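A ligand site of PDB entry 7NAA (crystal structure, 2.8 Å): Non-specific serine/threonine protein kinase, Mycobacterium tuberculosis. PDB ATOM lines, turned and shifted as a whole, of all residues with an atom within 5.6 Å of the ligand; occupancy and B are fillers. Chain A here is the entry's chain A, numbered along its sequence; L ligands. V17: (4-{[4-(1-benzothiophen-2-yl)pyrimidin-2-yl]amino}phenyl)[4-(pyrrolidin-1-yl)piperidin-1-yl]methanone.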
ATOM      1  N   ARG A  16      23.291   1.598  -6.786  1.00  0.00           N
ATOM      2  CA  ARG A  16      21.887   1.124  -6.622  1.00  0.00           C
ATOM      3  C   ARG A  16      21.816  -0.363  -6.987  1.00  0.00           C
ATOM      4  O   ARG A  16      22.738  -0.834  -7.647  1.00  0.00           O
ATOM      5  CB  ARG A  16      20.924   1.974  -7.458  1.00  0.00           C
ATOM      6  CG  ARG A  16      20.839   1.635  -8.938  1.00  0.00           C
ATOM      7  CD  ARG A  16      19.963   2.634  -9.668  1.00  0.00           C
ATOM      8  NE  ARG A  16      20.518   3.992  -9.641  1.00  0.00           N
ATOM      9  CZ  ARG A  16      20.866   4.714 -10.717  1.00  0.00           C
ATOM     10  NH1 ARG A  16      20.708   4.235 -11.939  1.00  0.00           N
ATOM     11  NH2 ARG A  16      21.355   5.938 -10.548  1.00  0.00           N
ATOM     12  N   GLN A  17      20.751  -1.070  -6.579  1.00  0.00           N
ATOM     13  CA  GLN A  17      20.406  -2.418  -7.119  1.00  0.00           C
ATOM     14  C   GLN A  17      19.708  -2.233  -8.476  1.00  0.00           C
ATOM     15  O   GLN A  17      18.833  -1.348  -8.566  1.00  0.00           O
ATOM     16  CB  GLN A  17      19.546  -3.215  -6.128  1.00  0.00           C
ATOM     17  N   LEU A  18      20.135  -2.988  -9.495  1.00  0.00           N
ATOM     18  CA  LEU A  18      19.593  -2.921 -10.883  1.00  0.00           C
ATOM     19  C   LEU A  18      18.605  -4.064 -11.108  1.00  0.00           C
ATOM     20  O   LEU A  18      17.711  -3.908 -11.964  1.00  0.00           O
ATOM     21  CB  LEU A  18      20.736  -3.061 -11.898  1.00  0.00           C
ATOM     22  CG  LEU A  18      21.668  -1.870 -12.072  1.00  0.00           C
ATOM     23  CD1 LEU A  18      22.801  -2.238 -13.019  1.00  0.00           C
ATOM     24  CD2 LEU A  18      20.913  -0.662 -12.594  1.00  0.00           C
ATOM     25  N   GLY A  19      18.772  -5.184 -10.425  1.00  0.00           N
ATOM     26  CA  GLY A  19      17.974  -6.395 -10.680  1.00  0.00           C
ATOM     27  C   GLY A  19      18.377  -7.564  -9.799  1.00  0.00           C
ATOM     28  O   GLY A  19      19.198  -7.375  -8.866  1.00  0.00           O
ATOM     29  N   SER A  20      17.787  -8.738 -10.067  1.00  0.00           N
ATOM     30  CA  SER A  20      17.896  -9.985  -9.252  1.00  0.00           C
ATOM     31  C   SER A  20      17.511 -11.201 -10.106  1.00  0.00           C
ATOM     32  O   SER A  20      18.424 -11.767 -10.769  1.00  0.00           O
ATOM     33  CB  SER A  20      17.042  -9.883  -7.987  1.00  0.00           C
ATOM     34  OG  SER A  20      17.201 -11.027  -7.161  1.00  0.00           O
ATOM     35  N   GLY A  24      21.581 -14.293  -6.922  1.00  0.00           N
ATOM     36  CA  GLY A  24      22.162 -13.347  -7.887  1.00  0.00           C
ATOM     37  C   GLY A  24      21.464 -11.993  -7.888  1.00  0.00           C
ATOM     38  O   GLY A  24      20.568 -11.790  -8.744  1.00  0.00           O
ATOM     39  N   VAL A  26      22.112  -7.929  -8.610  1.00  0.00           N
ATOM     40  CA  VAL A  26      22.962  -7.169  -9.585  1.00  0.00           C
ATOM     41  C   VAL A  26      22.913  -5.677  -9.251  1.00  0.00           C
ATOM     42  O   VAL A  26      21.820  -5.087  -9.377  1.00  0.00           O
ATOM     43  CB  VAL A  26      22.515  -7.417 -11.042  1.00  0.00           C
ATOM     44  CG1 VAL A  26      23.297  -6.566 -12.028  1.00  0.00           C
ATOM     45  CG2 VAL A  26      22.605  -8.891 -11.414  1.00  0.00           C
ATOM     46  N   ALA A  39      28.213  -3.124 -13.830  1.00  0.00           N
ATOM     47  CA  ALA A  39      27.175  -4.005 -13.264  1.00  0.00           C
ATOM     48  C   ALA A  39      27.877  -5.113 -12.472  1.00  0.00           C
ATOM     49  O   ALA A  39      28.619  -5.882 -13.097  1.00  0.00           O
ATOM     50  CB  ALA A  39      26.299  -4.552 -14.357  1.00  0.00           C
ATOM     51  N   LYS A  41      27.287  -8.422 -10.240  1.00  0.00           N
ATOM     52  CA  LYS A  41      26.384  -9.516  -9.794  1.00  0.00           C
ATOM     53  C   LYS A  41      26.998 -10.277  -8.631  1.00  0.00           C
ATOM     54  O   LYS A  41      28.151 -10.750  -8.780  1.00  0.00           O
ATOM     55  CB  LYS A  41      26.101 -10.499 -10.929  1.00  0.00           C
ATOM     56  CG  LYS A  41      25.058 -11.561 -10.625  1.00  0.00           C
ATOM     57  CD  LYS A  41      25.022 -12.607 -11.710  1.00  0.00           C
ATOM     58  CE  LYS A  41      23.661 -13.238 -11.897  1.00  0.00           C
ATOM     59  NZ  LYS A  41      23.715 -14.268 -12.970  1.00  0.00           N
ATOM     60  N   VAL A  73      26.479  -8.587 -23.353  1.00  0.00           N
ATOM     61  CA  VAL A  73      27.151  -7.785 -22.283  1.00  0.00           C
ATOM     62  C   VAL A  73      28.466  -8.475 -21.944  1.00  0.00           C
ATOM     63  O   VAL A  73      28.450  -9.702 -21.750  1.00  0.00           O
ATOM     64  CB  VAL A  73      26.211  -7.647 -21.064  1.00  0.00           C
ATOM     65  CG1 VAL A  73      26.894  -7.129 -19.825  1.00  0.00           C
ATOM     66  CG2 VAL A  73      25.021  -6.776 -21.410  1.00  0.00           C
ATOM     67  N   MET A  89      30.831  -6.829 -14.782  1.00  0.00           N
ATOM     68  CA  MET A  89      30.449  -6.816 -16.215  1.00  0.00           C
ATOM     69  C   MET A  89      30.087  -5.392 -16.647  1.00  0.00           C
ATOM     70  O   MET A  89      29.903  -4.541 -15.768  1.00  0.00           O
ATOM     71  CB  MET A  89      29.289  -7.783 -16.503  1.00  0.00           C
ATOM     72  CG  MET A  89      28.014  -7.481 -15.773  1.00  0.00           C
ATOM     73  SD  MET A  89      26.765  -8.775 -15.932  1.00  0.00           S
ATOM     74  CE  MET A  89      25.900  -8.564 -14.388  1.00  0.00           C
ATOM     75  N   ASP A  90      30.043  -5.146 -17.950  1.00  0.00           N
ATOM     76  CA  ASP A  90      29.605  -3.861 -18.555  1.00  0.00           C
ATOM     77  C   ASP A  90      28.277  -3.426 -17.927  1.00  0.00           C
ATOM     78  O   ASP A  90      27.433  -4.298 -17.753  1.00  0.00           O
ATOM     79  CB  ASP A  90      29.364  -3.999 -20.056  1.00  0.00           C
ATOM     80  CG  ASP A  90      30.583  -3.839 -20.916  1.00  0.00           C
ATOM     81  OD1 ASP A  90      31.535  -3.173 -20.450  1.00  0.00           O
ATOM     82  OD2 ASP A  90      30.539  -4.384 -22.051  1.00  0.00           O
ATOM     83  N   PHE A  91      28.126  -2.134 -17.643  1.00  0.00           N
ATOM     84  CA  PHE A  91      26.840  -1.501 -17.288  1.00  0.00           C
ATOM     85  C   PHE A  91      26.280  -0.864 -18.559  1.00  0.00           C
ATOM     86  O   PHE A  91      26.949   0.024 -19.127  1.00  0.00           O
ATOM     87  CB  PHE A  91      26.989  -0.439 -16.194  1.00  0.00           C
ATOM     88  CG  PHE A  91      25.841   0.526 -16.071  1.00  0.00           C
ATOM     89  CD1 PHE A  91      24.582   0.062 -15.727  1.00  0.00           C
ATOM     90  CD2 PHE A  91      26.005   1.878 -16.335  1.00  0.00           C
ATOM     91  CE1 PHE A  91      23.509   0.941 -15.627  1.00  0.00           C
ATOM     92  CE2 PHE A  91      24.930   2.755 -16.259  1.00  0.00           C
ATOM     93  CZ  PHE A  91      23.691   2.281 -15.895  1.00  0.00           C
ATOM     94  N   VAL A  92      25.092  -1.323 -18.983  1.00  0.00           N
ATOM     95  CA  VAL A  92      24.373  -0.762 -20.155  1.00  0.00           C
ATOM     96  C   VAL A  92      23.535   0.424 -19.671  1.00  0.00           C
ATOM     97  O   VAL A  92      22.470   0.228 -19.069  1.00  0.00           O
ATOM     98  CB  VAL A  92      23.524  -1.835 -20.855  1.00  0.00           C
ATOM     99  CG1 VAL A  92      22.922  -1.322 -22.156  1.00  0.00           C
ATOM    100  CG2 VAL A  92      24.316  -3.097 -21.097  1.00  0.00           C
ATOM    101  N   ASP A  93      24.044   1.632 -19.885  1.00  0.00           N
ATOM    102  CA  ASP A  93      23.427   2.914 -19.475  1.00  0.00           C
ATOM    103  C   ASP A  93      22.290   3.240 -20.437  1.00  0.00           C
ATOM    104  O   ASP A  93      22.533   3.827 -21.509  1.00  0.00           O
ATOM    105  CB  ASP A  93      24.492   4.000 -19.429  1.00  0.00           C
ATOM    106  CG  ASP A  93      24.006   5.308 -18.851  1.00  0.00           C
ATOM    107  OD1 ASP A  93      22.931   5.295 -18.165  1.00  0.00           O
ATOM    108  OD2 ASP A  93      24.697   6.318 -19.103  1.00  0.00           O
ATOM    109  N   GLY A  94      21.079   2.840 -20.029  1.00  0.00           N
ATOM    110  CA  GLY A  94      19.812   3.070 -20.749  1.00  0.00           C
ATOM    111  C   GLY A  94      18.653   2.504 -19.947  1.00  0.00           C
ATOM    112  O   GLY A  94      18.581   2.801 -18.742  1.00  0.00           O
ATOM    113  N   THR A  95      17.821   1.668 -20.576  1.00  0.00           N
ATOM    114  CA  THR A  95      16.636   1.018 -19.961  1.00  0.00           C
ATOM    115  C   THR A  95      16.653  -0.484 -20.267  1.00  0.00           C
ATOM    116  O   THR A  95      17.217  -0.866 -21.300  1.00  0.00           O
ATOM    117  CB  THR A  95      15.359   1.673 -20.494  1.00  0.00           C
ATOM    118  OG1 THR A  95      14.249   1.209 -19.705  1.00  0.00           O
ATOM    119  CG2 THR A  95      15.140   1.441 -21.964  1.00  0.00           C
ATOM    120  N   ASP A  96      16.047  -1.291 -19.399  1.00  0.00           N
ATOM    121  CA  ASP A  96      15.595  -2.666 -19.743  1.00  0.00           C
ATOM    122  C   ASP A  96      14.218  -2.544 -20.389  1.00  0.00           C
ATOM    123  O   ASP A  96      13.589  -1.470 -20.288  1.00  0.00           O
ATOM    124  CB  ASP A  96      15.594  -3.615 -18.539  1.00  0.00           C
ATOM    125  CG  ASP A  96      14.765  -3.146 -17.343  1.00  0.00           C
ATOM    126  OD1 ASP A  96      13.809  -2.385 -17.559  1.00  0.00           O
ATOM    127  OD2 ASP A  96      15.087  -3.572 -16.207  1.00  0.00           O
ATOM    128  N   VAL A  98      11.503  -4.070 -19.587  1.00  0.00           N
ATOM    129  CA  VAL A  98      10.488  -4.069 -18.476  1.00  0.00           C
ATOM    130  C   VAL A  98      10.008  -2.628 -18.257  1.00  0.00           C
ATOM    131  O   VAL A  98       8.796  -2.404 -18.319  1.00  0.00           O
ATOM    132  CB  VAL A  98      11.058  -4.678 -17.176  1.00  0.00           C
ATOM    133  CG1 VAL A  98      10.159  -4.407 -15.972  1.00  0.00           C
ATOM    134  CG2 VAL A  98      11.310  -6.164 -17.310  1.00  0.00           C
ATOM    135  N   SER A  99      10.952  -1.715 -18.007  1.00  0.00           N
ATOM    136  CA  SER A  99      10.726  -0.280 -17.723  1.00  0.00           C
ATOM    137  C   SER A  99      10.106   0.408 -18.932  1.00  0.00           C
ATOM    138  O   SER A  99       9.281   1.343 -18.734  1.00  0.00           O
ATOM    139  CB  SER A  99      11.996   0.397 -17.314  1.00  0.00           C
ATOM    140  OG  SER A  99      12.557  -0.271 -16.201  1.00  0.00           O
ATOM    141  N   LYS A 139      14.607 -13.049 -20.726  1.00  0.00           N
ATOM    142  CA  LYS A 139      13.411 -12.351 -20.187  1.00  0.00           C
ATOM    143  C   LYS A 139      13.569 -10.851 -20.390  1.00  0.00           C
ATOM    144  O   LYS A 139      14.686 -10.360 -20.494  1.00  0.00           O
ATOM    145  CB  LYS A 139      13.216 -12.707 -18.709  1.00  0.00           C
ATOM    146  CG  LYS A 139      14.341 -12.261 -17.802  1.00  0.00           C
ATOM    147  CD  LYS A 139      14.334 -12.915 -16.440  1.00  0.00           C
ATOM    148  CE  LYS A 139      15.439 -12.382 -15.559  1.00  0.00           C
ATOM    149  NZ  LYS A 139      15.383 -12.967 -14.207  1.00  0.00           N
ATOM    150  N   ALA A 141      13.835  -8.350 -18.593  1.00  0.00           N
ATOM    151  CA  ALA A 141      14.736  -7.657 -17.635  1.00  0.00           C
ATOM    152  C   ALA A 141      16.204  -7.865 -18.025  1.00  0.00           C
ATOM    153  O   ALA A 141      17.042  -7.074 -17.562  1.00  0.00           O
ATOM    154  CB  ALA A 141      14.464  -8.141 -16.230  1.00  0.00           C
ATOM    155  N   ASN A 142      16.493  -8.896 -18.834  1.00  0.00           N
ATOM    156  CA  ASN A 142      17.851  -9.217 -19.365  1.00  0.00           C
ATOM    157  C   ASN A 142      18.063  -8.576 -20.747  1.00  0.00           C
ATOM    158  O   ASN A 142      19.162  -8.778 -21.287  1.00  0.00           O
ATOM    159  CB  ASN A 142      18.073 -10.720 -19.482  1.00  0.00           C
ATOM    160  CG  ASN A 142      18.294 -11.359 -18.133  1.00  0.00           C
ATOM    161  OD1 ASN A 142      18.757 -10.683 -17.210  1.00  0.00           O
ATOM    162  ND2 ASN A 142      17.974 -12.644 -18.010  1.00  0.00           N
ATOM    163  N   LEU A 144      18.541  -5.199 -22.445  1.00  0.00           N
ATOM    164  CA  LEU A 144      18.908  -3.806 -22.137  1.00  0.00           C
ATOM    165  C   LEU A 144      19.084  -3.054 -23.457  1.00  0.00           C
ATOM    166  O   LEU A 144      19.440  -3.673 -24.445  1.00  0.00           O
ATOM    167  CB  LEU A 144      20.189  -3.822 -21.302  1.00  0.00           C
ATOM    168  CG  LEU A 144      20.129  -4.748 -20.087  1.00  0.00           C
ATOM    169  CD1 LEU A 144      21.469  -4.873 -19.400  1.00  0.00           C
ATOM    170  CD2 LEU A 144      19.123  -4.253 -19.101  1.00  0.00           C
ATOM    171  N   ALA A 158      21.940  -9.587 -21.444  1.00  0.00           N
ATOM    172  CA  ALA A 158      22.760  -9.672 -20.218  1.00  0.00           C
ATOM    173  C   ALA A 158      22.510 -10.989 -19.486  1.00  0.00           C
ATOM    174  O   ALA A 158      21.534 -11.665 -19.821  1.00  0.00           O
ATOM    175  CB  ALA A 158      22.520  -8.489 -19.333  1.00  0.00           C
ATOM    176  N   ASP A 159      23.414 -11.318 -18.569  1.00  0.00           N
ATOM    177  CA  ASP A 159      23.281 -12.409 -17.555  1.00  0.00           C
ATOM    178  C   ASP A 159      23.387 -13.778 -18.234  1.00  0.00           C
ATOM    179  O   ASP A 159      22.693 -14.711 -17.783  1.00  0.00           O
ATOM    180  CB  ASP A 159      21.979 -12.263 -16.749  1.00  0.00           C
ATOM    181  CG  ASP A 159      22.006 -13.032 -15.433  1.00  0.00           C
ATOM    182  OD1 ASP A 159      22.656 -12.539 -14.481  1.00  0.00           O
ATOM    183  OD2 ASP A 159      21.378 -14.102 -15.362  1.00  0.00           O
HETATM  184  C4  V17 L   1      14.676  -1.094 -12.494  1.00  0.00           C
HETATM  185  C14 V17 L   1      20.242  -0.209 -16.751  1.00  0.00           C
HETATM  186  C5  V17 L   1      14.337   0.342 -12.867  1.00  0.00           C
HETATM  187  C6  V17 L   1      14.801   0.657 -14.282  1.00  0.00           C
HETATM  188  C11 V17 L   1      18.263  -1.923 -15.863  1.00  0.00           C
HETATM  189  C7  V17 L   1      16.872  -0.214 -13.332  1.00  0.00           C
HETATM  190  C8  V17 L   1      16.184  -1.338 -12.563  1.00  0.00           C
HETATM  191  C9  V17 L   1      16.582  -0.059 -15.823  1.00  0.00           C
HETATM  192  C10 V17 L   1      17.964  -0.581 -16.041  1.00  0.00           C
HETATM  193  C12 V17 L   1      19.527  -2.421 -16.138  1.00  0.00           C
HETATM  194  C13 V17 L   1      20.531  -1.560 -16.588  1.00  0.00           C
HETATM  195  N1  V17 L   1      16.134   0.108 -14.558  1.00  0.00           N
HETATM  196  N2  V17 L   1      21.814  -2.022 -16.926  1.00  0.00           N
HETATM  197  C3  V17 L   1      12.575  -1.679 -11.187  1.00  0.00           C
HETATM  198  N3  V17 L   1      23.693  -3.271 -17.278  1.00  0.00           N
HETATM  199  O   V17 L   1      15.896   0.220 -16.787  1.00  0.00           O
HETATM  200  N   V17 L   1      14.028  -1.484 -11.222  1.00  0.00           N
HETATM  201  C2  V17 L   1      14.530  -2.436 -10.217  1.00  0.00           C
HETATM  202  C1  V17 L   1      13.663  -3.670 -10.398  1.00  0.00           C
HETATM  203  C   V17 L   1      12.388  -3.179 -11.059  1.00  0.00           C
HETATM  204  C15 V17 L   1      18.974   0.276 -16.479  1.00  0.00           C
HETATM  205  C16 V17 L   1      22.438  -3.241 -16.812  1.00  0.00           C
HETATM  206  N4  V17 L   1      21.751  -4.281 -16.286  1.00  0.00           N
HETATM  207  C19 V17 L   1      22.404  -5.445 -16.225  1.00  0.00           C
HETATM  208  C18 V17 L   1      23.706  -5.585 -16.668  1.00  0.00           C
HETATM  209  C17 V17 L   1      24.300  -4.458 -17.186  1.00  0.00           C
HETATM  210  C20 V17 L   1      21.644  -6.581 -15.712  1.00  0.00           C
HETATM  211  S   V17 L   1      19.922  -6.416 -15.519  1.00  0.00           S
HETATM  212  C27 V17 L   1      19.786  -8.033 -14.891  1.00  0.00           C
HETATM  213  C22 V17 L   1      21.042  -8.676 -14.828  1.00  0.00           C
HETATM  214  C21 V17 L   1      22.073  -7.800 -15.318  1.00  0.00           C
HETATM  215  C26 V17 L   1      18.634  -8.675 -14.454  1.00  0.00           C
HETATM  216  C25 V17 L   1      18.717  -9.960 -13.950  1.00  0.00           C
HETATM  217  C24 V17 L   1      19.943 -10.611 -13.874  1.00  0.00           C
HETATM  218  C23 V17 L   1      21.095  -9.970 -14.312  1.00  0.00           C
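N of Val 92 lies within hydrogen-bond range of N3 of the ligand (2.9 Å).
A nitrogen (N2) of the ligand sits at hydrogen-bond distance from the backbone carbonyl oxygen (O) of Val 92 (3.2 Å).
N of Asp 96 is in hydrogen-bond range of O of the ligand.
The side-chain hydroxyl (OG) of Ser 99 lies close to an oxygen (O) of the ligand (3.4 Å).
The side-chain hydroxyl (OG1) of Thr 95 sits close to an oxygen (O) of the ligand.
The backbone carbonyl oxygen of Ala 141 lies close to a sulfur (S) of the ligand (3.6 Å).
Leu 18 touches the ligand (O to C8, 3.0 Å).
O of Ser 20 touches C24 of the ligand (3.6 Å).
Val 26 touches the ligand.
CB of Ala 39 touches C17 of the ligand (3.5 Å).
O of Asp 90 touches C17 of the ligand (3.2 Å).
Phe 91 touches the ligand (CA to N3, 3.6 Å).
Gly 94 touches the ligand.
OD1 of Asn 142 touches C25 of the ligand (3.3 Å).
Leu 144 touches the ligand.
Asp 159 touches the ligand.
Hydrophobic or aromatic side chains within 4 Å of the ligand: Leu 18, Val 26, Ala 39, Phe 91, Val 92 and Leu 144.
15 residues have an atom within 4 Å of the ligand: Leu 18, Ser 20, Val 26, Ala 39, Asp 90, Phe 91, Val 92, Gly 94, Thr 95, Asp 96, Ser 99, Ala 141, Asn 142, Leu 144 and Asp 159.
The side-chain carboxylate of Asp 159 lies within salt-bridge range of the side-chain amino group of Lys 41, at 2.5 Å.
OD1 of Asp 96 is in hydrogen-bond range of OG of Ser 99 (2.8 Å).
N of Leu 18 lies within hydrogen-bond range of O of Val 26, 2.7 Å away.
The backbone carbonyl oxygen of Asn 142 sits at hydrogen-bond distance from the backbone NH of Ala 158, at 2.9 Å.
The backbone NH (N) of Val 26 is in hydrogen-bond range of the backbone carbonyl oxygen (O) of Gly 19 (3.0 Å).
The backbone carbonyl oxygen (O) of Met 89 sits at hydrogen-bond distance from the backbone NH (N) of Ala 39 (2.9 Å).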
